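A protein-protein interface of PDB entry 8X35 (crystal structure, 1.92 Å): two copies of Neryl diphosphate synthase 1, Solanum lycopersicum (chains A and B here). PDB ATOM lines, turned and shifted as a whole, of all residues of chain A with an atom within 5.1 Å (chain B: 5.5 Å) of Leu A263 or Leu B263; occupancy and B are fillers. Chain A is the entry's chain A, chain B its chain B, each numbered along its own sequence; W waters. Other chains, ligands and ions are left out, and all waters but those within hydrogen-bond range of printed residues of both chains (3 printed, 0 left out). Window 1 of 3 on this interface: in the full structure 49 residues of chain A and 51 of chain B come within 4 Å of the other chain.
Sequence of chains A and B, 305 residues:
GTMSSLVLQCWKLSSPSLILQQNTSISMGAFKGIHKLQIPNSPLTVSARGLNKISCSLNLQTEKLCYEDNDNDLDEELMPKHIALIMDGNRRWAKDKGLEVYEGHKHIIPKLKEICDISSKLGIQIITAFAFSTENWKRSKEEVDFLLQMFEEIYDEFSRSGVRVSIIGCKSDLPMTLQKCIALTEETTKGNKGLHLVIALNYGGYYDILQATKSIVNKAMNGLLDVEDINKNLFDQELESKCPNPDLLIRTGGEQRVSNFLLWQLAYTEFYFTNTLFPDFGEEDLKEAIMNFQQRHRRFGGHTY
The backbone NH of Asn A260 sits at hydrogen-bond distance from the backbone carbonyl oxygen of Ala B267 (2.9 Å). The backbone NH (N) of Asn B260 is in hydrogen-bond range of the backbone carbonyl oxygen (O) of Ala A267.
The backbone carbonyl oxygen of Asn A260 lies within hydrogen-bond range of the backbone NH of Gly A205, 3.0 Å away. OD1 of Asn A260 sits at hydrogen-bond distance from N of Tyr A206. The backbone NH of Gly B205 lies within hydrogen-bond range of the backbone carbonyl oxygen of Asn B260 (3.0 Å). The side-chain amide oxygen of Asn B260 is in hydrogen-bond range of the backbone NH of Tyr B206.
Tyr A206 touches Trp B264 (CD1 to CZ2, 3.6 Å). Tyr A206 touches Ala B267 (OH to CB, 3.3 Å). Trp B264 touches Ile A209 (CZ3 to CG2, 3.9 Å). CG2 of Val A258 touches O of Leu B266 (3.8 Å). Val A258 touches Ala B267. Leu A263 touches Leu B263. CA of Ala B267 touches CD2 of Leu A263, 3.9 Å away. Trp A264 touches Tyr B206 (CE2 to CE1, 3.5 Å). Ala A267 touches Tyr B206. CG2 of Val B258 touches O of Ala A267, at 3.8 Å.
Of chain B, only Leu B263 and Ala B267 come within 4 Å of Leu A263. Leu B263 touches two residues of chain A. Of the printed residues of chain A, Val B258 touches Ala A267 (3.8 Å). Of the printed residues of chain A, Trp B264 touches Tyr A206 and Ile A209. Printed residues of chain A within 4 Å of Asn B260: Ala A267 (2.9 Å). Of the printed residues of chain B, Ile A209 touches Trp B264 (3.9 Å). Printed residues of chain A within 4 Å of Leu B266: Val A258. The nearest residue of chain A that does not touch Leu B263 is Trp A264 (4.2 Å).
Hydrophobic or aromatic side chains of chain B that line the printed part of chain A: Tyr B206, Ile B209, Val B258, Leu B263, Trp B264 and Ala B267. Of the 12 printed residues of chain A, 7 touch a printed residue of chain B. Among the printed residues, 14 pairs touch across the chains. Among the printed residues, no Asp or Glu carboxylate lies within 4 Å of a Lys or Arg side-chain nitrogen of the other chain.
Tyr A206 touches Trp B264, and with the chains exchanged Trp A264 touches Tyr B206. Val A258 touches Leu B266, but with the chains exchanged Leu A266 does not touch Val B258 (4.03 Å). Val A258 touches Ala B267, and with the chains exchanged Ala A267 touches Val B258. Leu A263 touches Ala B267, and with the chains exchanged Ala A267 touches Leu B263. 12 positions are printed for both chains.
Water W3 lies within hydrogen-bond range of OH of Tyr A206 (2.5 Å), O of Trp B264 (2.7 Å), O of Gln B265 (3.2 Å) and N of Ala B267 (3.4 Å). Water W1 lies within hydrogen-bond range of N of Val A258 (2.8 Å), O of Leu B266 (2.9 Å) and O of Ala B267 (3.3 Å). Water W2 lies within hydrogen-bond range of the backbone carbonyl oxygen (O) of Leu A266 (2.9 Å), the backbone NH (N) of Val B258 (3.0 Å) and the backbone carbonyl oxygen (O) of Ala A267 (3.3 Å).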
ATOM      1  N   GLY A 205      34.021 -16.478  -3.116  1.00  0.00           N
ATOM      2  CA  GLY A 205      33.107 -16.485  -1.993  1.00  0.00           C
ATOM      3  C   GLY A 205      33.748 -15.981  -0.702  1.00  0.00           C
ATOM      4  O   GLY A 205      33.083 -15.335   0.114  1.00  0.00           O
ATOM      5  N   TYR A 206      35.019 -16.331  -0.464  1.00  0.00           N
ATOM      6  CA  TYR A 206      35.726 -15.807   0.706  1.00  0.00           C
ATOM      7  C   TYR A 206      35.748 -14.284   0.664  1.00  0.00           C
ATOM      8  O   TYR A 206      35.375 -13.611   1.626  1.00  0.00           O
ATOM      9  CB  TYR A 206      37.174 -16.285   0.741  1.00  0.00           C
ATOM     10  CG  TYR A 206      37.477 -17.743   0.877  1.00  0.00           C
ATOM     11  CD1 TYR A 206      36.807 -18.551   1.781  1.00  0.00           C
ATOM     12  CD2 TYR A 206      38.522 -18.288   0.161  1.00  0.00           C
ATOM     13  CE1 TYR A 206      37.133 -19.912   1.911  1.00  0.00           C
ATOM     14  CE2 TYR A 206      38.864 -19.625   0.297  1.00  0.00           C
ATOM     15  CZ  TYR A 206      38.170 -20.429   1.166  1.00  0.00           C
ATOM     16  OH  TYR A 206      38.529 -21.770   1.278  1.00  0.00           O
ATOM     17  N   ILE A 209      32.290 -12.684   1.458  1.00  0.00           N
ATOM     18  CA  ILE A 209      31.927 -12.743   2.873  1.00  0.00           C
ATOM     19  C   ILE A 209      32.812 -11.807   3.689  1.00  0.00           C
ATOM     20  O   ILE A 209      32.340 -11.138   4.615  1.00  0.00           O
ATOM     21  CB  ILE A 209      32.011 -14.195   3.384  1.00  0.00           C
ATOM     22  CG1 ILE A 209      30.872 -15.026   2.785  1.00  0.00           C
ATOM     23  CG2 ILE A 209      32.021 -14.248   4.960  1.00  0.00           C
ATOM     24  CD1 ILE A 209      31.146 -16.542   2.701  1.00  0.00           C
ATOM     25  N   VAL A 258      32.819 -26.527  -6.190  1.00  0.00           N
ATOM     26  CA  VAL A 258      32.348 -25.162  -6.470  1.00  0.00           C
ATOM     27  C   VAL A 258      33.480 -24.155  -6.666  1.00  0.00           C
ATOM     28  O   VAL A 258      33.221 -23.040  -7.164  1.00  0.00           O
ATOM     29  CB  VAL A 258      31.361 -24.674  -5.384  1.00  0.00           C
ATOM     30  CG1 VAL A 258      30.130 -25.570  -5.384  1.00  0.00           C
ATOM     31  CG2 VAL A 258      32.007 -24.587  -3.959  1.00  0.00           C
ATOM     32  N   ASN A 260      35.324 -22.050  -4.889  1.00  0.00           N
ATOM     33  CA  ASN A 260      35.242 -20.701  -4.280  1.00  0.00           C
ATOM     34  C   ASN A 260      34.373 -19.714  -5.084  1.00  0.00           C
ATOM     35  O   ASN A 260      34.687 -18.521  -5.173  1.00  0.00           O
ATOM     36  CB  ASN A 260      36.651 -20.113  -4.066  1.00  0.00           C
ATOM     37  CG  ASN A 260      36.670 -18.913  -3.090  1.00  0.00           C
ATOM     38  OD1 ASN A 260      35.871 -18.830  -2.148  1.00  0.00           O
ATOM     39  ND2 ASN A 260      37.602 -17.992  -3.313  1.00  0.00           N
ATOM     40  N   PHE A 261      33.265 -20.201  -5.663  1.00  0.00           N
ATOM     41  CA  PHE A 261      32.224 -19.355  -6.265  1.00  0.00           C
ATOM     42  C   PHE A 261      31.300 -18.797  -5.174  1.00  0.00           C
ATOM     43  O   PHE A 261      31.789 -18.323  -4.148  1.00  0.00           O
ATOM     44  CB  PHE A 261      31.476 -20.178  -7.336  1.00  0.00           C
ATOM     45  CG  PHE A 261      30.696 -19.372  -8.353  1.00  0.00           C
ATOM     46  CD1 PHE A 261      30.971 -18.028  -8.600  1.00  0.00           C
ATOM     47  CD2 PHE A 261      29.682 -19.990  -9.081  1.00  0.00           C
ATOM     48  CE1 PHE A 261      30.233 -17.300  -9.560  1.00  0.00           C
ATOM     49  CE2 PHE A 261      28.953 -19.288 -10.041  1.00  0.00           C
ATOM     50  CZ  PHE A 261      29.227 -17.930 -10.281  1.00  0.00           C
ATOM     51  N   LEU A 262      29.977 -18.838  -5.354  1.00  0.00           N
ATOM     52  CA  LEU A 262      29.015 -18.159  -4.458  1.00  0.00           C
ATOM     53  C   LEU A 262      28.685 -18.962  -3.184  1.00  0.00           C
ATOM     54  O   LEU A 262      27.563 -19.443  -3.006  1.00  0.00           O
ATOM     55  CB  LEU A 262      27.725 -17.893  -5.231  1.00  0.00           C
ATOM     56  CG  LEU A 262      27.775 -17.137  -6.553  1.00  0.00           C
ATOM     57  CD1 LEU A 262      26.479 -17.296  -7.381  1.00  0.00           C
ATOM     58  CD2 LEU A 262      28.034 -15.670  -6.254  1.00  0.00           C
ATOM     59  N   LEU A 263      29.636 -19.003  -2.229  1.00  0.00           N
ATOM     60  CA  LEU A 263      29.514 -19.919  -1.085  1.00  0.00           C
ATOM     61  C   LEU A 263      28.240 -19.678  -0.261  1.00  0.00           C
ATOM     62  O   LEU A 263      27.461 -20.606  -0.024  1.00  0.00           O
ATOM     63  CB  LEU A 263      30.762 -19.833  -0.190  1.00  0.00           C
ATOM     64  CG  LEU A 263      32.100 -20.127  -0.888  1.00  0.00           C
ATOM     65  CD1 LEU A 263      33.263 -19.998   0.103  1.00  0.00           C
ATOM     66  CD2 LEU A 263      32.083 -21.521  -1.467  1.00  0.00           C
ATOM     67  N   TRP A 264      28.030 -18.455   0.229  1.00  0.00           N
ATOM     68  CA  TRP A 264      26.843 -18.177   1.045  1.00  0.00           C
ATOM     69  C   TRP A 264      25.561 -18.369   0.229  1.00  0.00           C
ATOM     70  O   TRP A 264      24.563 -18.893   0.729  1.00  0.00           O
ATOM     71  CB  TRP A 264      26.921 -16.746   1.591  1.00  0.00           C
ATOM     72  CG  TRP A 264      25.677 -16.177   2.245  1.00  0.00           C
ATOM     73  CD1 TRP A 264      24.555 -15.706   1.618  1.00  0.00           C
ATOM     74  CD2 TRP A 264      25.470 -15.950   3.660  1.00  0.00           C
ATOM     75  NE1 TRP A 264      23.655 -15.219   2.550  1.00  0.00           N
ATOM     76  CE2 TRP A 264      24.196 -15.358   3.808  1.00  0.00           C
ATOM     77  CE3 TRP A 264      26.243 -16.185   4.811  1.00  0.00           C
ATOM     78  CZ2 TRP A 264      23.669 -15.007   5.071  1.00  0.00           C
ATOM     79  CZ3 TRP A 264      25.715 -15.844   6.065  1.00  0.00           C
ATOM     80  CH2 TRP A 264      24.443 -15.260   6.180  1.00  0.00           C
ATOM     81  N   GLN A 265      25.578 -17.941  -1.026  1.00  0.00           N
ATOM     82  CA  GLN A 265      24.385 -17.927  -1.857  1.00  0.00           C
ATOM     83  C   GLN A 265      23.951 -19.317  -2.343  1.00  0.00           C
ATOM     84  O   GLN A 265      22.819 -19.459  -2.814  1.00  0.00           O
ATOM     85  CB  GLN A 265      24.632 -16.984  -3.036  1.00  0.00           C
ATOM     86  CG  GLN A 265      24.940 -15.543  -2.580  1.00  0.00           C
ATOM     87  CD  GLN A 265      26.412 -15.248  -2.323  1.00  0.00           C
ATOM     88  OE1 GLN A 265      27.243 -16.149  -2.248  1.00  0.00           O
ATOM     89  NE2 GLN A 265      26.749 -13.937  -2.209  1.00  0.00           N
ATOM     90  N   LEU A 266      24.793 -20.346  -2.232  1.00  0.00           N
ATOM     91  CA  LEU A 266      24.466 -21.655  -2.782  1.00  0.00           C
ATOM     92  C   LEU A 266      23.969 -22.633  -1.707  1.00  0.00           C
ATOM     93  O   LEU A 266      23.971 -23.839  -1.944  1.00  0.00           O
ATOM     94  CB  LEU A 266      25.686 -22.233  -3.506  1.00  0.00           C
ATOM     95  CG  LEU A 266      26.153 -21.554  -4.809  1.00  0.00           C
ATOM     96  CD1 LEU A 266      27.470 -22.132  -5.283  1.00  0.00           C
ATOM     97  CD2 LEU A 266      25.102 -21.732  -5.933  1.00  0.00           C
ATOM     98  N   ALA A 267      23.519 -22.128  -0.551  1.00  0.00           N
ATOM     99  CA  ALA A 267      23.224 -22.994   0.596  1.00  0.00           C
ATOM    100  C   ALA A 267      22.119 -24.006   0.293  1.00  0.00           C
ATOM    101  O   ALA A 267      22.155 -25.140   0.802  1.00  0.00           O
ATOM    102  CB  ALA A 267      22.824 -22.133   1.805  1.00  0.00           C
ATOM    103  N   GLY B 205      25.520 -23.569   8.122  1.00  0.00           N
ATOM    104  CA  GLY B 205      26.560 -22.729   7.561  1.00  0.00           C
ATOM    105  C   GLY B 205      26.326 -21.247   7.784  1.00  0.00           C
ATOM    106  O   GLY B 205      27.271 -20.506   8.078  1.00  0.00           O
ATOM    107  N   TYR B 206      25.078 -20.780   7.621  1.00  0.00           N
ATOM    108  CA  TYR B 206      24.747 -19.396   7.993  1.00  0.00           C
ATOM    109  C   TYR B 206      25.086 -19.110   9.455  1.00  0.00           C
ATOM    110  O   TYR B 206      25.611 -18.035   9.788  1.00  0.00           O
ATOM    111  CB  TYR B 206      23.261 -19.101   7.787  1.00  0.00           C
ATOM    112  CG  TYR B 206      22.731 -19.166   6.366  1.00  0.00           C
ATOM    113  CD1 TYR B 206      23.434 -18.602   5.322  1.00  0.00           C
ATOM    114  CD2 TYR B 206      21.500 -19.763   6.093  1.00  0.00           C
ATOM    115  CE1 TYR B 206      22.934 -18.653   3.996  1.00  0.00           C
ATOM    116  CE2 TYR B 206      20.992 -19.813   4.796  1.00  0.00           C
ATOM    117  CZ  TYR B 206      21.714 -19.266   3.755  1.00  0.00           C
ATOM    118  OH  TYR B 206      21.202 -19.329   2.466  1.00  0.00           O
ATOM    119  N   ILE B 209      28.998 -18.649  10.045  1.00  0.00           N
ATOM    120  CA  ILE B 209      29.471 -17.344   9.549  1.00  0.00           C
ATOM    121  C   ILE B 209      28.942 -16.189  10.404  1.00  0.00           C
ATOM    122  O   ILE B 209      29.665 -15.215  10.684  1.00  0.00           O
ATOM    123  CB  ILE B 209      29.087 -17.175   8.063  1.00  0.00           C
ATOM    124  CG1 ILE B 209      29.866 -18.168   7.200  1.00  0.00           C
ATOM    125  CG2 ILE B 209      29.299 -15.724   7.600  1.00  0.00           C
ATOM    126  CD1 ILE B 209      29.279 -18.335   5.781  1.00  0.00           C
ATOM    127  N   VAL B 258      23.939 -29.066  -0.779  1.00  0.00           N
ATOM    128  CA  VAL B 258      24.583 -29.080   0.541  1.00  0.00           C
ATOM    129  C   VAL B 258      23.659 -28.693   1.682  1.00  0.00           C
ATOM    130  O   VAL B 258      24.025 -28.919   2.854  1.00  0.00           O
ATOM    131  CB  VAL B 258      25.861 -28.214   0.581  1.00  0.00           C
ATOM    132  CG1 VAL B 258      26.911 -28.746  -0.384  1.00  0.00           C
ATOM    133  CG2 VAL B 258      25.554 -26.730   0.371  1.00  0.00           C
ATOM    134  N   ASN B 260      22.691 -26.046   3.490  1.00  0.00           N
ATOM    135  CA  ASN B 260      23.127 -25.203   4.617  1.00  0.00           C
ATOM    136  C   ASN B 260      23.962 -25.972   5.649  1.00  0.00           C
ATOM    137  O   ASN B 260      23.852 -25.717   6.848  1.00  0.00           O
ATOM    138  CB  ASN B 260      21.939 -24.517   5.302  1.00  0.00           C
ATOM    139  CG  ASN B 260      22.383 -23.403   6.295  1.00  0.00           C
ATOM    140  OD1 ASN B 260      23.363 -22.686   6.059  1.00  0.00           O
ATOM    141  ND2 ASN B 260      21.639 -23.255   7.384  1.00  0.00           N
ATOM    142  N   PHE B 261      24.806 -26.914   5.181  1.00  0.00           N
ATOM    143  CA  PHE B 261      25.804 -27.601   6.015  1.00  0.00           C
ATOM    144  C   PHE B 261      27.014 -26.681   6.025  1.00  0.00           C
ATOM    145  O   PHE B 261      26.875 -25.466   6.148  1.00  0.00           O
ATOM    146  CB  PHE B 261      26.156 -29.007   5.454  1.00  0.00           C
ATOM    147  CG  PHE B 261      27.044 -29.907   6.375  1.00  0.00           C
ATOM    148  CD1 PHE B 261      27.054 -29.771   7.755  1.00  0.00           C
ATOM    149  CD2 PHE B 261      27.833 -30.924   5.817  1.00  0.00           C
ATOM    150  CE1 PHE B 261      27.849 -30.627   8.577  1.00  0.00           C
ATOM    151  CE2 PHE B 261      28.629 -31.774   6.616  1.00  0.00           C
ATOM    152  CZ  PHE B 261      28.625 -31.627   8.003  1.00  0.00           C
ATOM    153  N   LEU B 262      28.205 -27.211   5.848  1.00  0.00           N
ATOM    154  CA  LEU B 262      29.333 -26.318   5.782  1.00  0.00           C
ATOM    155  C   LEU B 262      29.147 -25.459   4.529  1.00  0.00           C
ATOM    156  O   LEU B 262      28.624 -25.928   3.515  1.00  0.00           O
ATOM    157  CB  LEU B 262      30.608 -27.157   5.767  1.00  0.00           C
ATOM    158  CG  LEU B 262      30.554 -28.229   6.870  1.00  0.00           C
ATOM    159  CD1 LEU B 262      31.730 -29.200   6.799  1.00  0.00           C
ATOM    160  CD2 LEU B 262      30.495 -27.585   8.245  1.00  0.00           C
ATOM    161  N   LEU B 263      29.398 -24.165   4.641  1.00  0.00           N
ATOM    162  CA  LEU B 263      29.442 -23.304   3.458  1.00  0.00           C
ATOM    163  C   LEU B 263      30.848 -22.772   3.227  1.00  0.00           C
ATOM    164  O   LEU B 263      31.449 -23.028   2.185  1.00  0.00           O
ATOM    165  CB  LEU B 263      28.444 -22.141   3.578  1.00  0.00           C
ATOM    166  CG  LEU B 263      26.968 -22.508   3.664  1.00  0.00           C
ATOM    167  CD1 LEU B 263      26.127 -21.264   3.831  1.00  0.00           C
ATOM    168  CD2 LEU B 263      26.537 -23.313   2.412  1.00  0.00           C
ATOM    169  N   TRP B 264      31.398 -22.045   4.197  1.00  0.00           N
ATOM    170  CA  TRP B 264      32.733 -21.475   4.047  1.00  0.00           C
ATOM    171  C   TRP B 264      33.774 -22.564   3.818  1.00  0.00           C
ATOM    172  O   TRP B 264      34.692 -22.412   3.001  1.00  0.00           O
ATOM    173  CB  TRP B 264      33.047 -20.661   5.308  1.00  0.00           C
ATOM    174  CG  TRP B 264      34.461 -20.171   5.425  1.00  0.00           C
ATOM    175  CD1 TRP B 264      35.552 -20.906   5.803  1.00  0.00           C
ATOM    176  CD2 TRP B 264      34.941 -18.840   5.167  1.00  0.00           C
ATOM    177  NE1 TRP B 264      36.678 -20.127   5.780  1.00  0.00           N
ATOM    178  CE2 TRP B 264      36.334 -18.852   5.400  1.00  0.00           C
ATOM    179  CE3 TRP B 264      34.333 -17.646   4.750  1.00  0.00           C
ATOM    180  CZ2 TRP B 264      37.135 -17.711   5.243  1.00  0.00           C
ATOM    181  CZ3 TRP B 264      35.133 -16.502   4.589  1.00  0.00           C
ATOM    182  CH2 TRP B 264      36.518 -16.545   4.847  1.00  0.00           C
ATOM    183  N   GLN B 265      33.653 -23.665   4.551  1.00  0.00           N
ATOM    184  CA  GLN B 265      34.644 -24.729   4.560  1.00  0.00           C
ATOM    185  C   GLN B 265      34.676 -25.565   3.279  1.00  0.00           C
ATOM    186  O   GLN B 265      35.657 -26.281   3.068  1.00  0.00           O
ATOM    187  CB  GLN B 265      34.387 -25.617   5.787  1.00  0.00           C
ATOM    188  CG  GLN B 265      34.501 -24.867   7.139  1.00  0.00           C
ATOM    189  CD  GLN B 265      33.208 -24.183   7.576  1.00  0.00           C
ATOM    190  OE1 GLN B 265      32.213 -24.159   6.845  1.00  0.00           O
ATOM    191  NE2 GLN B 265      33.229 -23.601   8.768  1.00  0.00           N
ATOM    192  N   LEU B 266      33.679 -25.465   2.395  1.00  0.00           N
ATOM    193  CA  LEU B 266      33.602 -26.361   1.235  1.00  0.00           C
ATOM    194  C   LEU B 266      34.135 -25.749  -0.062  1.00  0.00           C
ATOM    195  O   LEU B 266      33.940 -26.338  -1.143  1.00  0.00           O
ATOM    196  CB  LEU B 266      32.157 -26.834   1.032  1.00  0.00           C
ATOM    197  CG  LEU B 266      31.520 -27.703   2.140  1.00  0.00           C
ATOM    198  CD1 LEU B 266      30.047 -27.957   1.837  1.00  0.00           C
ATOM    199  CD2 LEU B 266      32.254 -29.010   2.385  1.00  0.00           C
ATOM    200  N   ALA B 267      34.842 -24.612   0.019  1.00  0.00           N
ATOM    201  CA  ALA B 267      35.211 -23.841  -1.177  1.00  0.00           C
ATOM    202  C   ALA B 267      35.904 -24.694  -2.236  1.00  0.00           C
ATOM    203  O   ALA B 267      35.629 -24.534  -3.430  1.00  0.00           O
ATOM    204  CB  ALA B 267      36.105 -22.652  -0.781  1.00  0.00           C
HETATM  205  O   HOH W   1      33.970 -27.363  -3.803  1.00  0.00           O
HETATM  206  O   HOH W   2      22.955 -26.576  -2.050  1.00  0.00           O
HETATM  207  O   HOH W   3      37.075 -23.499   2.375  1.00  0.00           O
